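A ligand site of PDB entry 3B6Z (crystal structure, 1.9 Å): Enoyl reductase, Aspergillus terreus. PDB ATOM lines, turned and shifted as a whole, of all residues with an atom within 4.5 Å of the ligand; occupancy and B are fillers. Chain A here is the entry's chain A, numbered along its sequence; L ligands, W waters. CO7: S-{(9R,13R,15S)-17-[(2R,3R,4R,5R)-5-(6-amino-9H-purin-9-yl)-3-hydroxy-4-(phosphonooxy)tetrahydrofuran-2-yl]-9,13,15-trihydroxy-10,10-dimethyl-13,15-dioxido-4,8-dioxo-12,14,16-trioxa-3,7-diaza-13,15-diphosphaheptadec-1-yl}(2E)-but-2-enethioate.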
ATOM      1  N   PRO A  50       6.578 -20.573 -13.296  1.00  0.00           N
ATOM      2  CA  PRO A  50       6.549 -21.026 -14.693  1.00  0.00           C
ATOM      3  C   PRO A  50       7.943 -21.394 -15.219  1.00  0.00           C
ATOM      4  O   PRO A  50       8.067 -22.300 -16.027  1.00  0.00           O
ATOM      5  CB  PRO A  50       5.953 -19.828 -15.446  1.00  0.00           C
ATOM      6  CG  PRO A  50       5.091 -19.108 -14.417  1.00  0.00           C
ATOM      7  CD  PRO A  50       5.836 -19.297 -13.100  1.00  0.00           C
ATOM      8  N   SER A  51       8.990 -20.703 -14.766  1.00  0.00           N
ATOM      9  CA  SER A  51      10.346 -21.021 -15.268  1.00  0.00           C
ATOM     10  C   SER A  51      10.724 -22.494 -15.003  1.00  0.00           C
ATOM     11  O   SER A  51      11.425 -23.125 -15.829  1.00  0.00           O
ATOM     12  CB  SER A  51      11.380 -20.069 -14.657  1.00  0.00           C
ATOM     13  OG  SER A  51      11.194 -20.015 -13.246  1.00  0.00           O
ATOM     14  N   LYS A  54       9.511 -24.803 -17.671  1.00  0.00           N
ATOM     15  CA  LYS A  54      10.119 -24.625 -18.977  1.00  0.00           C
ATOM     16  C   LYS A  54      11.510 -25.232 -19.042  1.00  0.00           C
ATOM     17  O   LYS A  54      12.128 -25.181 -20.090  1.00  0.00           O
ATOM     18  CB  LYS A  54      10.169 -23.146 -19.364  1.00  0.00           C
ATOM     19  CG  LYS A  54       8.808 -22.494 -19.446  1.00  0.00           C
ATOM     20  CD  LYS A  54       8.961 -20.991 -19.563  1.00  0.00           C
ATOM     21  CE  LYS A  54       7.648 -20.278 -19.284  1.00  0.00           C
ATOM     22  NZ  LYS A  54       6.632 -20.530 -20.348  1.00  0.00           N
ATOM     23  N   THR A  68      13.555 -22.744  -7.998  1.00  0.00           N
ATOM     24  CA  THR A  68      14.117 -21.441  -7.682  1.00  0.00           C
ATOM     25  C   THR A  68      13.806 -21.070  -6.218  1.00  0.00           C
ATOM     26  O   THR A  68      14.721 -20.732  -5.466  1.00  0.00           O
ATOM     27  CB  THR A  68      13.510 -20.351  -8.626  1.00  0.00           C
ATOM     28  OG1 THR A  68      13.949 -20.573  -9.980  1.00  0.00           O
ATOM     29  CG2 THR A  68      13.957 -18.966  -8.225  1.00  0.00           C
ATOM     30  N   ALA A  93      16.477 -17.568  -3.174  1.00  0.00           N
ATOM     31  CA  ALA A  93      16.396 -18.137  -4.519  1.00  0.00           C
ATOM     32  C   ALA A  93      17.605 -19.007  -4.829  1.00  0.00           C
ATOM     33  O   ALA A  93      18.733 -18.726  -4.431  1.00  0.00           O
ATOM     34  CB  ALA A  93      16.282 -16.997  -5.566  1.00  0.00           C
ATOM     35  N   GLN A  94      17.339 -20.072  -5.584  1.00  0.00           N
ATOM     36  CA  GLN A  94      18.385 -20.860  -6.194  1.00  0.00           C
ATOM     37  C   GLN A  94      18.419 -20.604  -7.695  1.00  0.00           C
ATOM     38  O   GLN A  94      17.515 -19.960  -8.274  1.00  0.00           O
ATOM     39  CB  GLN A  94      18.181 -22.349  -5.900  1.00  0.00           C
ATOM     40  CG  GLN A  94      18.967 -22.869  -4.675  1.00  0.00           C
ATOM     41  CD  GLN A  94      20.470 -22.856  -4.904  1.00  0.00           C
ATOM     42  OE1 GLN A  94      21.241 -23.027  -3.971  1.00  0.00           O
ATOM     43  NE2 GLN A  94      20.883 -22.633  -6.144  1.00  0.00           N
ATOM     44  N   ALA A 135      11.648 -15.376  -6.128  1.00  0.00           N
ATOM     45  CA  ALA A 135      11.719 -15.086  -7.553  1.00  0.00           C
ATOM     46  C   ALA A 135      10.985 -13.748  -7.826  1.00  0.00           C
ATOM     47  O   ALA A 135      11.397 -12.976  -8.694  1.00  0.00           O
ATOM     48  CB  ALA A 135      11.084 -16.232  -8.359  1.00  0.00           C
ATOM     49  N   SER A 138      13.283 -10.829  -6.740  1.00  0.00           N
ATOM     50  CA  SER A 138      14.408 -10.780  -7.623  1.00  0.00           C
ATOM     51  C   SER A 138      14.000 -10.233  -8.994  1.00  0.00           C
ATOM     52  O   SER A 138      14.699  -9.379  -9.562  1.00  0.00           O
ATOM     53  CB  SER A 138      15.003 -12.195  -7.768  1.00  0.00           C
ATOM     54  OG  SER A 138      15.497 -12.651  -6.505  1.00  0.00           O
ATOM     55  N   THR A 139      12.869 -10.714  -9.504  1.00  0.00           N
ATOM     56  CA  THR A 139      12.418 -10.326 -10.845  1.00  0.00           C
ATOM     57  C   THR A 139      11.999  -8.846 -10.851  1.00  0.00           C
ATOM     58  O   THR A 139      12.357  -8.111 -11.777  1.00  0.00           O
ATOM     59  CB  THR A 139      11.280 -11.229 -11.382  1.00  0.00           C
ATOM     60  OG1 THR A 139      11.759 -12.565 -11.397  1.00  0.00           O
ATOM     61  CG2 THR A 139      10.934 -10.854 -12.819  1.00  0.00           C
ATOM     62  N   LEU A 142      15.152  -6.700 -10.919  1.00  0.00           N
ATOM     63  CA  LEU A 142      15.779  -6.657 -12.235  1.00  0.00           C
ATOM     64  C   LEU A 142      14.970  -5.801 -13.191  1.00  0.00           C
ATOM     65  O   LEU A 142      15.552  -5.089 -14.006  1.00  0.00           O
ATOM     66  CB  LEU A 142      15.972  -8.055 -12.842  1.00  0.00           C
ATOM     67  CG  LEU A 142      16.976  -8.969 -12.125  1.00  0.00           C
ATOM     68  CD1 LEU A 142      17.011 -10.342 -12.767  1.00  0.00           C
ATOM     69  CD2 LEU A 142      18.360  -8.307 -12.078  1.00  0.00           C
ATOM     70  N   TYR A 171       1.621  -4.690 -17.774  1.00  0.00           N
ATOM     71  CA  TYR A 171       0.781  -5.598 -18.550  1.00  0.00           C
ATOM     72  C   TYR A 171       0.852  -6.968 -17.878  1.00  0.00           C
ATOM     73  O   TYR A 171       1.921  -7.585 -17.810  1.00  0.00           O
ATOM     74  CB  TYR A 171       1.229  -5.666 -20.025  1.00  0.00           C
ATOM     75  CG  TYR A 171       0.180  -6.285 -20.933  1.00  0.00           C
ATOM     76  CD1 TYR A 171      -0.766  -5.487 -21.601  1.00  0.00           C
ATOM     77  CD2 TYR A 171       0.101  -7.677 -21.086  1.00  0.00           C
ATOM     78  CE1 TYR A 171      -1.764  -6.073 -22.436  1.00  0.00           C
ATOM     79  CE2 TYR A 171      -0.890  -8.275 -21.922  1.00  0.00           C
ATOM     80  CZ  TYR A 171      -1.814  -7.466 -22.567  1.00  0.00           C
ATOM     81  OH  TYR A 171      -2.761  -8.073 -23.379  1.00  0.00           O
ATOM     82  N   SER A 174      -1.975  -9.156 -12.510  1.00  0.00           N
ATOM     83  CA  SER A 174      -2.304 -10.206 -11.541  1.00  0.00           C
ATOM     84  C   SER A 174      -1.205 -11.300 -11.451  1.00  0.00           C
ATOM     85  O   SER A 174      -1.326 -12.266 -10.649  1.00  0.00           O
ATOM     86  CB  SER A 174      -3.672 -10.849 -11.856  1.00  0.00           C
ATOM     87  OG  SER A 174      -3.577 -11.718 -12.961  1.00  0.00           O
ATOM     88  N   THR A 175      -0.171 -11.184 -12.290  1.00  0.00           N
ATOM     89  CA  THR A 175       0.935 -12.147 -12.251  1.00  0.00           C
ATOM     90  C   THR A 175       1.671 -12.055 -10.911  1.00  0.00           C
ATOM     91  O   THR A 175       1.715 -10.987 -10.309  1.00  0.00           O
ATOM     92  CB  THR A 175       1.936 -11.931 -13.375  1.00  0.00           C
ATOM     93  OG1 THR A 175       2.541 -10.649 -13.240  1.00  0.00           O
ATOM     94  CG2 THR A 175       1.275 -12.048 -14.783  1.00  0.00           C
ATOM     95  N   ALA A 176       2.278 -13.151 -10.469  1.00  0.00           N
ATOM     96  CA  ALA A 176       3.163 -13.165  -9.302  1.00  0.00           C
ATOM     97  C   ALA A 176       4.208 -12.029  -9.348  1.00  0.00           C
ATOM     98  O   ALA A 176       4.430 -11.318  -8.368  1.00  0.00           O
ATOM     99  CB  ALA A 176       3.831 -14.541  -9.151  1.00  0.00           C
ATOM    100  N   THR A 177       4.841 -11.831 -10.494  1.00  0.00           N
ATOM    101  CA  THR A 177       5.858 -10.773 -10.609  1.00  0.00           C
ATOM    102  C   THR A 177       5.251  -9.377 -10.405  1.00  0.00           C
ATOM    103  O   THR A 177       5.839  -8.540  -9.686  1.00  0.00           O
ATOM    104  CB  THR A 177       6.597 -10.828 -11.948  1.00  0.00           C
ATOM    105  OG1 THR A 177       7.166 -12.130 -12.157  1.00  0.00           O
ATOM    106  CG2 THR A 177       7.731  -9.722 -11.994  1.00  0.00           C
ATOM    107  N   CYS A 196      -5.378  -6.797 -16.552  1.00  0.00           N
ATOM    108  CA  CYS A 196      -5.526  -8.202 -16.144  1.00  0.00           C
ATOM    109  C   CYS A 196      -7.000  -8.580 -16.315  1.00  0.00           C
ATOM    110  O   CYS A 196      -7.734  -7.842 -16.943  1.00  0.00           O
ATOM    111  CB  CYS A 196      -5.001  -8.431 -14.696  1.00  0.00           C
ATOM    112  SG  CYS A 196      -5.931  -7.651 -13.352  1.00  0.00           S
ATOM    113  N   SER A 197      -7.420  -9.749 -15.827  1.00  0.00           N
ATOM    114  CA  SER A 197      -8.827 -10.149 -15.950  1.00  0.00           C
ATOM    115  C   SER A 197      -9.585  -9.550 -14.795  1.00  0.00           C
ATOM    116  O   SER A 197      -8.978  -9.417 -13.718  1.00  0.00           O
ATOM    117  CB  SER A 197      -8.977 -11.679 -15.898  1.00  0.00           C
ATOM    118  OG  SER A 197      -8.380 -12.249 -17.050  1.00  0.00           O
ATOM    119  N   HIS A 199     -11.734 -10.511 -12.551  1.00  0.00           N
ATOM    120  CA  HIS A 199     -11.802 -11.177 -11.245  1.00  0.00           C
ATOM    121  C   HIS A 199     -10.538 -10.930 -10.387  1.00  0.00           C
ATOM    122  O   HIS A 199     -10.573 -11.102  -9.166  1.00  0.00           O
ATOM    123  CB  HIS A 199     -12.148 -12.661 -11.382  1.00  0.00           C
ATOM    124  CG  HIS A 199     -10.986 -13.515 -11.722  1.00  0.00           C
ATOM    125  ND1 HIS A 199     -10.250 -14.177 -10.764  1.00  0.00           N
ATOM    126  CD2 HIS A 199     -10.401 -13.803 -12.913  1.00  0.00           C
ATOM    127  CE1 HIS A 199      -9.271 -14.842 -11.349  1.00  0.00           C
ATOM    128  NE2 HIS A 199      -9.342 -14.636 -12.656  1.00  0.00           N
ATOM    129  N   ASN A 200      -9.453 -10.495 -11.002  1.00  0.00           N
ATOM    130  CA  ASN A 200      -8.250 -10.094 -10.275  1.00  0.00           C
ATOM    131  C   ASN A 200      -8.087  -8.586 -10.135  1.00  0.00           C
ATOM    132  O   ASN A 200      -7.044  -8.129  -9.674  1.00  0.00           O
ATOM    133  CB  ASN A 200      -6.999 -10.676 -10.936  1.00  0.00           C
ATOM    134  CG  ASN A 200      -6.900 -12.191 -10.765  1.00  0.00           C
ATOM    135  OD1 ASN A 200      -7.151 -12.734  -9.703  1.00  0.00           O
ATOM    136  ND2 ASN A 200      -6.500 -12.868 -11.812  1.00  0.00           N
ATOM    137  N   TYR A 215      -7.559  -6.385 -20.069  1.00  0.00           N
ATOM    138  CA  TYR A 215      -6.691  -6.350 -21.244  1.00  0.00           C
ATOM    139  C   TYR A 215      -7.435  -6.697 -22.537  1.00  0.00           C
ATOM    140  O   TYR A 215      -6.948  -6.424 -23.629  1.00  0.00           O
ATOM    141  CB  TYR A 215      -5.470  -7.289 -21.066  1.00  0.00           C
ATOM    142  CG  TYR A 215      -5.791  -8.782 -21.094  1.00  0.00           C
ATOM    143  CD1 TYR A 215      -5.816  -9.501 -22.302  1.00  0.00           C
ATOM    144  CD2 TYR A 215      -6.088  -9.475 -19.912  1.00  0.00           C
ATOM    145  CE1 TYR A 215      -6.108 -10.854 -22.329  1.00  0.00           C
ATOM    146  CE2 TYR A 215      -6.397 -10.855 -19.949  1.00  0.00           C
ATOM    147  CZ  TYR A 215      -6.405 -11.522 -21.148  1.00  0.00           C
ATOM    148  OH  TYR A 215      -6.681 -12.883 -21.173  1.00  0.00           O
ATOM    149  N   CYS A 238       4.607  -8.367 -18.235  1.00  0.00           N
ATOM    150  CA  CYS A 238       4.727  -9.601 -17.446  1.00  0.00           C
ATOM    151  C   CYS A 238       4.060 -10.819 -18.090  1.00  0.00           C
ATOM    152  O   CYS A 238       3.925 -11.857 -17.434  1.00  0.00           O
ATOM    153  CB  CYS A 238       4.124  -9.421 -16.045  1.00  0.00           C
ATOM    154  SG  CYS A 238       4.885  -8.141 -15.036  1.00  0.00           S
ATOM    155  N   ILE A 239       3.594 -10.660 -19.336  1.00  0.00           N
ATOM    156  CA  ILE A 239       2.875 -11.715 -20.054  1.00  0.00           C
ATOM    157  C   ILE A 239       3.809 -12.242 -21.111  1.00  0.00           C
ATOM    158  O   ILE A 239       3.998 -13.445 -21.230  1.00  0.00           O
ATOM    159  CB  ILE A 239       1.489 -11.198 -20.641  1.00  0.00           C
ATOM    160  CG1 ILE A 239       0.538 -10.786 -19.494  1.00  0.00           C
ATOM    161  CG2 ILE A 239       0.869 -12.215 -21.647  1.00  0.00           C
ATOM    162  CD1 ILE A 239       0.307 -11.887 -18.392  1.00  0.00           C
ATOM    163  N   THR A 240       4.371 -11.322 -21.894  1.00  0.00           N
ATOM    164  CA  THR A 240       5.503 -11.546 -22.805  1.00  0.00           C
ATOM    165  C   THR A 240       5.158 -12.341 -24.073  1.00  0.00           C
ATOM    166  O   THR A 240       5.869 -13.253 -24.443  1.00  0.00           O
ATOM    167  CB  THR A 240       6.788 -12.165 -22.057  1.00  0.00           C
ATOM    168  OG1 THR A 240       6.674 -13.602 -21.983  1.00  0.00           O
ATOM    169  CG2 THR A 240       6.923 -11.626 -20.652  1.00  0.00           C
ATOM    170  N   ASN A 241       4.049 -12.035 -24.726  1.00  0.00           N
ATOM    171  CA  ASN A 241       3.774 -12.725 -25.983  1.00  0.00           C
ATOM    172  C   ASN A 241       3.542 -11.714 -27.102  1.00  0.00           C
ATOM    173  O   ASN A 241       3.729 -10.518 -26.883  1.00  0.00           O
ATOM    174  CB  ASN A 241       2.592 -13.694 -25.822  1.00  0.00           C
ATOM    175  CG  ASN A 241       1.315 -12.977 -25.421  1.00  0.00           C
ATOM    176  OD1 ASN A 241       1.169 -11.783 -25.629  1.00  0.00           O
ATOM    177  ND2 ASN A 241       0.407 -13.709 -24.834  1.00  0.00           N
ATOM    178  N   LEU A 262       9.739  -9.858 -19.449  1.00  0.00           N
ATOM    179  CA  LEU A 262      10.327 -10.872 -18.568  1.00  0.00           C
ATOM    180  C   LEU A 262      10.882 -12.076 -19.370  1.00  0.00           C
ATOM    181  O   LEU A 262      11.467 -13.005 -18.799  1.00  0.00           O
ATOM    182  CB  LEU A 262       9.305 -11.294 -17.495  1.00  0.00           C
ATOM    183  CG  LEU A 262       8.691 -10.164 -16.620  1.00  0.00           C
ATOM    184  CD1 LEU A 262       7.754 -10.797 -15.556  1.00  0.00           C
ATOM    185  CD2 LEU A 262       9.770  -9.263 -15.956  1.00  0.00           C
ATOM    186  N   ASN A 263      10.742 -12.041 -20.688  1.00  0.00           N
ATOM    187  CA  ASN A 263      11.330 -13.072 -21.548  1.00  0.00           C
ATOM    188  C   ASN A 263      11.902 -12.412 -22.772  1.00  0.00           C
ATOM    189  O   ASN A 263      11.562 -11.262 -23.039  1.00  0.00           O
ATOM    190  CB  ASN A 263      10.231 -14.073 -22.007  1.00  0.00           C
ATOM    191  CG  ASN A 263      10.043 -15.230 -21.033  1.00  0.00           C
ATOM    192  OD1 ASN A 263      10.977 -15.989 -20.777  1.00  0.00           O
ATOM    193  ND2 ASN A 263       8.817 -15.387 -20.520  1.00  0.00           N
ATOM    194  N   THR A 280      14.522  -9.260 -18.811  1.00  0.00           N
ATOM    195  CA  THR A 280      15.183  -9.720 -17.604  1.00  0.00           C
ATOM    196  C   THR A 280      15.765 -11.117 -17.770  1.00  0.00           C
ATOM    197  O   THR A 280      15.026 -12.064 -18.082  1.00  0.00           O
ATOM    198  CB  THR A 280      14.211  -9.735 -16.406  1.00  0.00           C
ATOM    199  OG1 THR A 280      13.109 -10.591 -16.723  1.00  0.00           O
ATOM    200  CG2 THR A 280      13.677  -8.338 -16.079  1.00  0.00           C
ATOM    201  N   GLY A 282      17.149 -13.870 -15.540  1.00  0.00           N
ATOM    202  CA  GLY A 282      17.086 -14.279 -14.117  1.00  0.00           C
ATOM    203  C   GLY A 282      18.382 -14.492 -13.330  1.00  0.00           C
ATOM    204  O   GLY A 282      18.525 -13.908 -12.271  1.00  0.00           O
ATOM    205  N   HIS A 327       2.466 -12.745  -2.869  1.00  0.00           N
ATOM    206  CA  HIS A 327       1.338 -13.017  -3.765  1.00  0.00           C
ATOM    207  C   HIS A 327       0.384 -14.022  -3.064  1.00  0.00           C
ATOM    208  O   HIS A 327       0.853 -14.826  -2.308  1.00  0.00           O
ATOM    209  CB  HIS A 327       1.930 -13.631  -5.033  1.00  0.00           C
ATOM    210  CG  HIS A 327       1.026 -13.529  -6.216  1.00  0.00           C
ATOM    211  ND1 HIS A 327       0.586 -14.643  -6.914  1.00  0.00           N
ATOM    212  CD2 HIS A 327       0.482 -12.459  -6.819  1.00  0.00           C
ATOM    213  CE1 HIS A 327      -0.196 -14.244  -7.904  1.00  0.00           C
ATOM    214  NE2 HIS A 327      -0.280 -12.925  -7.852  1.00  0.00           N
ATOM    215  N   LEU A 351      -3.589 -21.684 -12.969  1.00  0.00           N
ATOM    216  CA  LEU A 351      -3.530 -20.812 -11.794  1.00  0.00           C
ATOM    217  C   LEU A 351      -3.754 -19.355 -12.188  1.00  0.00           C
ATOM    218  O   LEU A 351      -3.145 -18.839 -13.136  1.00  0.00           O
ATOM    219  CB  LEU A 351      -2.198 -20.962 -11.036  1.00  0.00           C
ATOM    220  CG  LEU A 351      -1.992 -22.201 -10.151  1.00  0.00           C
ATOM    221  CD1 LEU A 351      -0.724 -22.034  -9.407  1.00  0.00           C
ATOM    222  CD2 LEU A 351      -3.125 -22.361  -9.175  1.00  0.00           C
ATOM    223  N   SER A 352      -4.668 -18.711 -11.457  1.00  0.00           N
ATOM    224  CA  SER A 352      -4.926 -17.294 -11.667  1.00  0.00           C
ATOM    225  C   SER A 352      -5.012 -16.592 -10.335  1.00  0.00           C
ATOM    226  O   SER A 352      -5.802 -16.986  -9.473  1.00  0.00           O
ATOM    227  CB  SER A 352      -6.198 -17.072 -12.499  1.00  0.00           C
ATOM    228  OG  SER A 352      -6.568 -15.700 -12.539  1.00  0.00           O
ATOM    229  N   GLY A 353      -4.161 -15.578 -10.166  1.00  0.00           N
ATOM    230  CA  GLY A 353      -4.136 -14.718  -8.980  1.00  0.00           C
ATOM    231  C   GLY A 353      -3.577 -15.390  -7.726  1.00  0.00           C
ATOM    232  O   GLY A 353      -3.767 -14.889  -6.621  1.00  0.00           O
ATOM    233  N   LYS A 355      -0.197 -18.206  -6.154  1.00  0.00           N
ATOM    234  CA  LYS A 355       1.083 -18.871  -6.319  1.00  0.00           C
ATOM    235  C   LYS A 355       1.018 -20.271  -5.658  1.00  0.00           C
ATOM    236  O   LYS A 355       0.591 -20.412  -4.537  1.00  0.00           O
ATOM    237  CB  LYS A 355       2.220 -18.015  -5.710  1.00  0.00           C
ATOM    238  CG  LYS A 355       3.652 -18.592  -5.863  1.00  0.00           C
ATOM    239  CD  LYS A 355       4.518 -17.582  -6.563  1.00  0.00           C
ATOM    240  CE  LYS A 355       5.731 -18.201  -7.131  1.00  0.00           C
ATOM    241  NZ  LYS A 355       6.145 -17.468  -8.364  1.00  0.00           N
HETATM  242  O1  CO7 L   1      14.562 -13.047 -12.420  1.00  0.00           O
HETATM  243  C1  CO7 L   1      14.359 -14.239 -12.121  1.00  0.00           C
HETATM  244  C2  CO7 L   1      14.835 -14.799 -10.818  1.00  0.00           C
HETATM  245  C3  CO7 L   1      14.766 -16.095 -10.494  1.00  0.00           C
HETATM  246  C4  CO7 L   1      15.336 -16.463  -9.148  1.00  0.00           C
HETATM  247  S1  CO7 L   1      13.539 -15.178 -13.227  1.00  0.00           S
HETATM  248  C5  CO7 L   1      13.485 -13.996 -14.592  1.00  0.00           C
HETATM  249  C6  CO7 L   1      12.056 -13.732 -15.104  1.00  0.00           C
HETATM  250  N1  CO7 L   1      11.721 -14.570 -16.267  1.00  0.00           N
HETATM  251  C7  CO7 L   1      11.367 -15.869 -16.305  1.00  0.00           C
HETATM  252  O2  CO7 L   1      11.303 -16.545 -15.284  1.00  0.00           O
HETATM  253  C8  CO7 L   1      11.044 -16.523 -17.649  1.00  0.00           C
HETATM  254  C9  CO7 L   1      10.142 -17.778 -17.517  1.00  0.00           C
HETATM  255  N2  CO7 L   1       8.879 -17.328 -16.948  1.00  0.00           N
HETATM  256  C10 CO7 L   1       7.772 -16.988 -17.593  1.00  0.00           C
HETATM  257  O3  CO7 L   1       7.698 -17.052 -18.811  1.00  0.00           O
HETATM  258  C11 CO7 L   1       6.588 -16.517 -16.782  1.00  0.00           C
HETATM  259  O4  CO7 L   1       5.343 -16.971 -17.353  1.00  0.00           O
HETATM  260  C12 CO7 L   1       6.570 -14.989 -16.579  1.00  0.00           C
HETATM  261  C13 CO7 L   1       6.358 -14.233 -17.884  1.00  0.00           C
HETATM  262  C14 CO7 L   1       7.862 -14.558 -15.875  1.00  0.00           C
HETATM  263  C15 CO7 L   1       5.367 -14.697 -15.708  1.00  0.00           C
HETATM  264  O5  CO7 L   1       5.433 -15.498 -14.525  1.00  0.00           O
HETATM  265  P1  CO7 L   1       4.701 -15.028 -13.183  1.00  0.00           P
HETATM  266  O6  CO7 L   1       5.051 -13.612 -12.859  1.00  0.00           O
HETATM  267  O7  CO7 L   1       5.043 -16.082 -12.164  1.00  0.00           O
HETATM  268  O8  CO7 L   1       3.108 -14.976 -13.454  1.00  0.00           O
HETATM  269  P2  CO7 L   1       1.916 -15.976 -13.058  1.00  0.00           P
HETATM  270  O9  CO7 L   1       2.207 -17.352 -13.606  1.00  0.00           O
HETATM  271  O10 CO7 L   1       1.485 -15.780 -11.625  1.00  0.00           O
HETATM  272  O11 CO7 L   1       0.799 -15.309 -14.006  1.00  0.00           O
HETATM  273  C16 CO7 L   1      -0.303 -16.005 -14.594  1.00  0.00           C
HETATM  274  C17 CO7 L   1      -1.336 -14.952 -14.960  1.00  0.00           C
HETATM  275  C18 CO7 L   1      -2.688 -15.572 -15.221  1.00  0.00           C
HETATM  276  O12 CO7 L   1      -3.387 -15.683 -13.998  1.00  0.00           O
HETATM  277  C19 CO7 L   1      -3.401 -14.580 -16.123  1.00  0.00           C
HETATM  278  O13 CO7 L   1      -3.962 -13.537 -15.321  1.00  0.00           O
HETATM  279  P3  CO7 L   1      -5.550 -13.144 -15.375  1.00  0.00           P
HETATM  280  O14 CO7 L   1      -6.242 -14.390 -14.883  1.00  0.00           O
HETATM  281  O15 CO7 L   1      -5.683 -12.017 -14.394  1.00  0.00           O
HETATM  282  O16 CO7 L   1      -5.846 -12.748 -16.817  1.00  0.00           O
HETATM  283  O17 CO7 L   1      -1.047 -14.437 -16.243  1.00  0.00           O
HETATM  284  C20 CO7 L   1      -2.266 -13.982 -16.891  1.00  0.00           C
HETATM  285  N3  CO7 L   1      -2.228 -14.411 -18.310  1.00  0.00           N
HETATM  286  C21 CO7 L   1      -2.475 -13.636 -19.358  1.00  0.00           C
HETATM  287  N4  CO7 L   1      -2.822 -12.313 -19.447  1.00  0.00           N
HETATM  288  C22 CO7 L   1      -3.013 -11.765 -20.658  1.00  0.00           C
HETATM  289  C23 CO7 L   1      -1.870 -15.638 -18.779  1.00  0.00           C
HETATM  290  N5  CO7 L   1      -1.912 -15.641 -20.140  1.00  0.00           N
HETATM  291  C24 CO7 L   1      -2.278 -14.392 -20.518  1.00  0.00           C
HETATM  292  C25 CO7 L   1      -2.478 -13.765 -21.758  1.00  0.00           C
HETATM  293  N6  CO7 L   1      -2.859 -12.466 -21.786  1.00  0.00           N
HETATM  294  N7  CO7 L   1      -2.329 -14.408 -22.928  1.00  0.00           N
HETATM  295  O   HOH W   1       2.759 -17.309 -16.618  1.00  0.00           O
HETATM  296  O   HOH W   2      -3.880 -10.679 -17.403  1.00  0.00           O
HETATM  297  O   HOH W   3      -0.840 -15.435 -10.608  1.00  0.00           O
HETATM  298  O   HOH W   4      -6.062 -14.151 -18.998  1.00  0.00           O
HETATM  299  O   HOH W   5       1.680 -17.563  -9.640  1.00  0.00           O
HETATM  300  O   HOH W   6       5.154 -16.775 -20.549  1.00  0.00           O
HETATM  301  O   HOH W   7       4.153 -17.786 -10.331  1.00  0.00           O
HETATM  302  O   HOH W   8      -2.338 -10.609 -15.090  1.00  0.00           O
HETATM  303  O   HOH W   9       9.002 -17.823 -13.901  1.00  0.00           O
HETATM  304  O   HOH W  10       7.866 -16.607 -11.827  1.00  0.00           O
HETATM  305  O   HOH W  11      -2.557 -12.956 -25.619  1.00  0.00           O
HETATM  306  O   HOH W  12      -2.328 -10.705 -23.809  1.00  0.00           O
HETATM  307  O   HOH W  13       1.852 -14.878 -17.516  1.00  0.00           O
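An oxygen (O15) of the ligand lies within hydrogen-bond range of the side-chain hydroxyl (OG) of Ser 174 (2.6 Å). O15 of the ligand is in hydrogen-bond range of N of Ser 197 (3.2 Å). An oxygen (O16) of the ligand is in hydrogen-bond range of the side-chain hydroxyl (OG) of Ser 197, at 2.6 Å. An oxygen (O3) of the ligand sits at hydrogen-bond distance from the side-chain amide nitrogen (ND2) of Asn 263, at 2.6 Å. N of Thr 177 is in hydrogen-bond range of O6 of the ligand, at 3.0 Å. The side-chain hydroxyl (OG1) of Thr 177 is in hydrogen-bond range of an oxygen (O6) of the ligand (2.7 Å). The side-chain hydroxyl of Ser 352 lies within hydrogen-bond range of an oxygen (O14) of the ligand (2.7 Å). The side-chain amide nitrogen (ND2) of Asn 200 is in hydrogen-bond range of an oxygen (O15) of the ligand (2.8 Å). The backbone NH (N) of Ala 176 sits at hydrogen-bond distance from an oxygen (O10) of the ligand. A nitrogen (N1) of the ligand lies within hydrogen-bond range of the backbone carbonyl oxygen (O) of Leu 262 (3.0 Å). The side-chain hydroxyl of Thr 139 sits at hydrogen-bond distance from an oxygen (O1) of the ligand (3.0 Å). The backbone carbonyl oxygen of Leu 351 lies within hydrogen-bond range of an oxygen (O12) of the ligand (3.3 Å). The side-chain amide nitrogen (ND2) of Asn 241 sits close to a nitrogen (N7) of the ligand, at 3.4 Å.
ND2 of Asn 200 sits at hydrogen-bond distance from OG of Ser 174, 3.3 Å away. The backbone carbonyl oxygen of Ser 174 is in hydrogen-bond range of a ring nitrogen (NE2) of His 327, 3.1 Å away. The side-chain amide nitrogen (ND2) of Asn 263 sits at hydrogen-bond distance from the side-chain hydroxyl (OG1) of Thr 240. The side-chain hydroxyl (OG) of Ser 352 sits at hydrogen-bond distance from the side-chain amide nitrogen (ND2) of Asn 200, 2.9 Å away. OG of Ser 352 sits at hydrogen-bond distance from NE2 of His 199 (3.0 Å). The side-chain amide nitrogen of Asn 200 sits close to a ring nitrogen (NE2) of His 199, at 3.5 Å. The backbone carbonyl oxygen (O) of Thr 68 is in hydrogen-bond range of the backbone NH (N) of Gln 94 (2.7 Å). O of Cys 196 sits at hydrogen-bond distance from N of Tyr 215 (3.5 Å).
Residues that only touch the ligand: Thr 68 (3.0 Å), Lys 54 (3.3 Å), Thr 175 (3.3 Å), Gly 282 (3.3 Å), Ile 239 (3.3 Å), Cys 238 (3.4 Å), Tyr 215 (3.4 Å), Pro 50 (3.4 Å), Ser 51 (3.6 Å), Cys 196 (3.7 Å), Leu 142 (3.7 Å), Thr 280 (3.7 Å), Ala 93 (3.7 Å), His 199 (3.8 Å), Thr 240 (3.8 Å) and Gly 353 (3.9 Å). Hydrophobic or aromatic side chains within 4 Å of the ligand: Pro 50, Ala 93, Leu 142, Ala 176, Tyr 215, Ile 239 and Leu 262. 27 residues have an atom within 4 Å of the ligand: Pro 50, Ser 51, Lys 54, Thr 68, Ala 93, Thr 139, Leu 142, Ser 174, Thr 175, Ala 176, Thr 177, Cys 196, Ser 197, His 199, Asn 200, Tyr 215, Cys 238, Ile 239, Thr 240, Asn 241, Leu 262, Asn 263, Thr 280, Gly 282, Leu 351, Ser 352 and Gly 353. The nearest printed residue that does not touch the ligand is Ser 138 (4.01 Å).
Water W4 bridges OH of Tyr 215 and O16 of the ligand. Water W7 bridges O7 of the ligand (2.7 Å) and NZ of Lys 355 (2.8 Å). Water W12 bridges OH of Tyr 171 (2.7 Å) and N6 of the ligand (2.7 Å). Water W9 lies within hydrogen-bond range of an oxygen (O2) of the ligand (3.0 Å) and the backbone NH of Ser 51 (3.0 Å). Water W11 lies within hydrogen-bond range of N7 of the ligand and ND2 of Asn 241. Water W8 lies within hydrogen-bond range of OG of Ser 174 (2.7 Å) and O13 of the ligand (3.4 Å).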
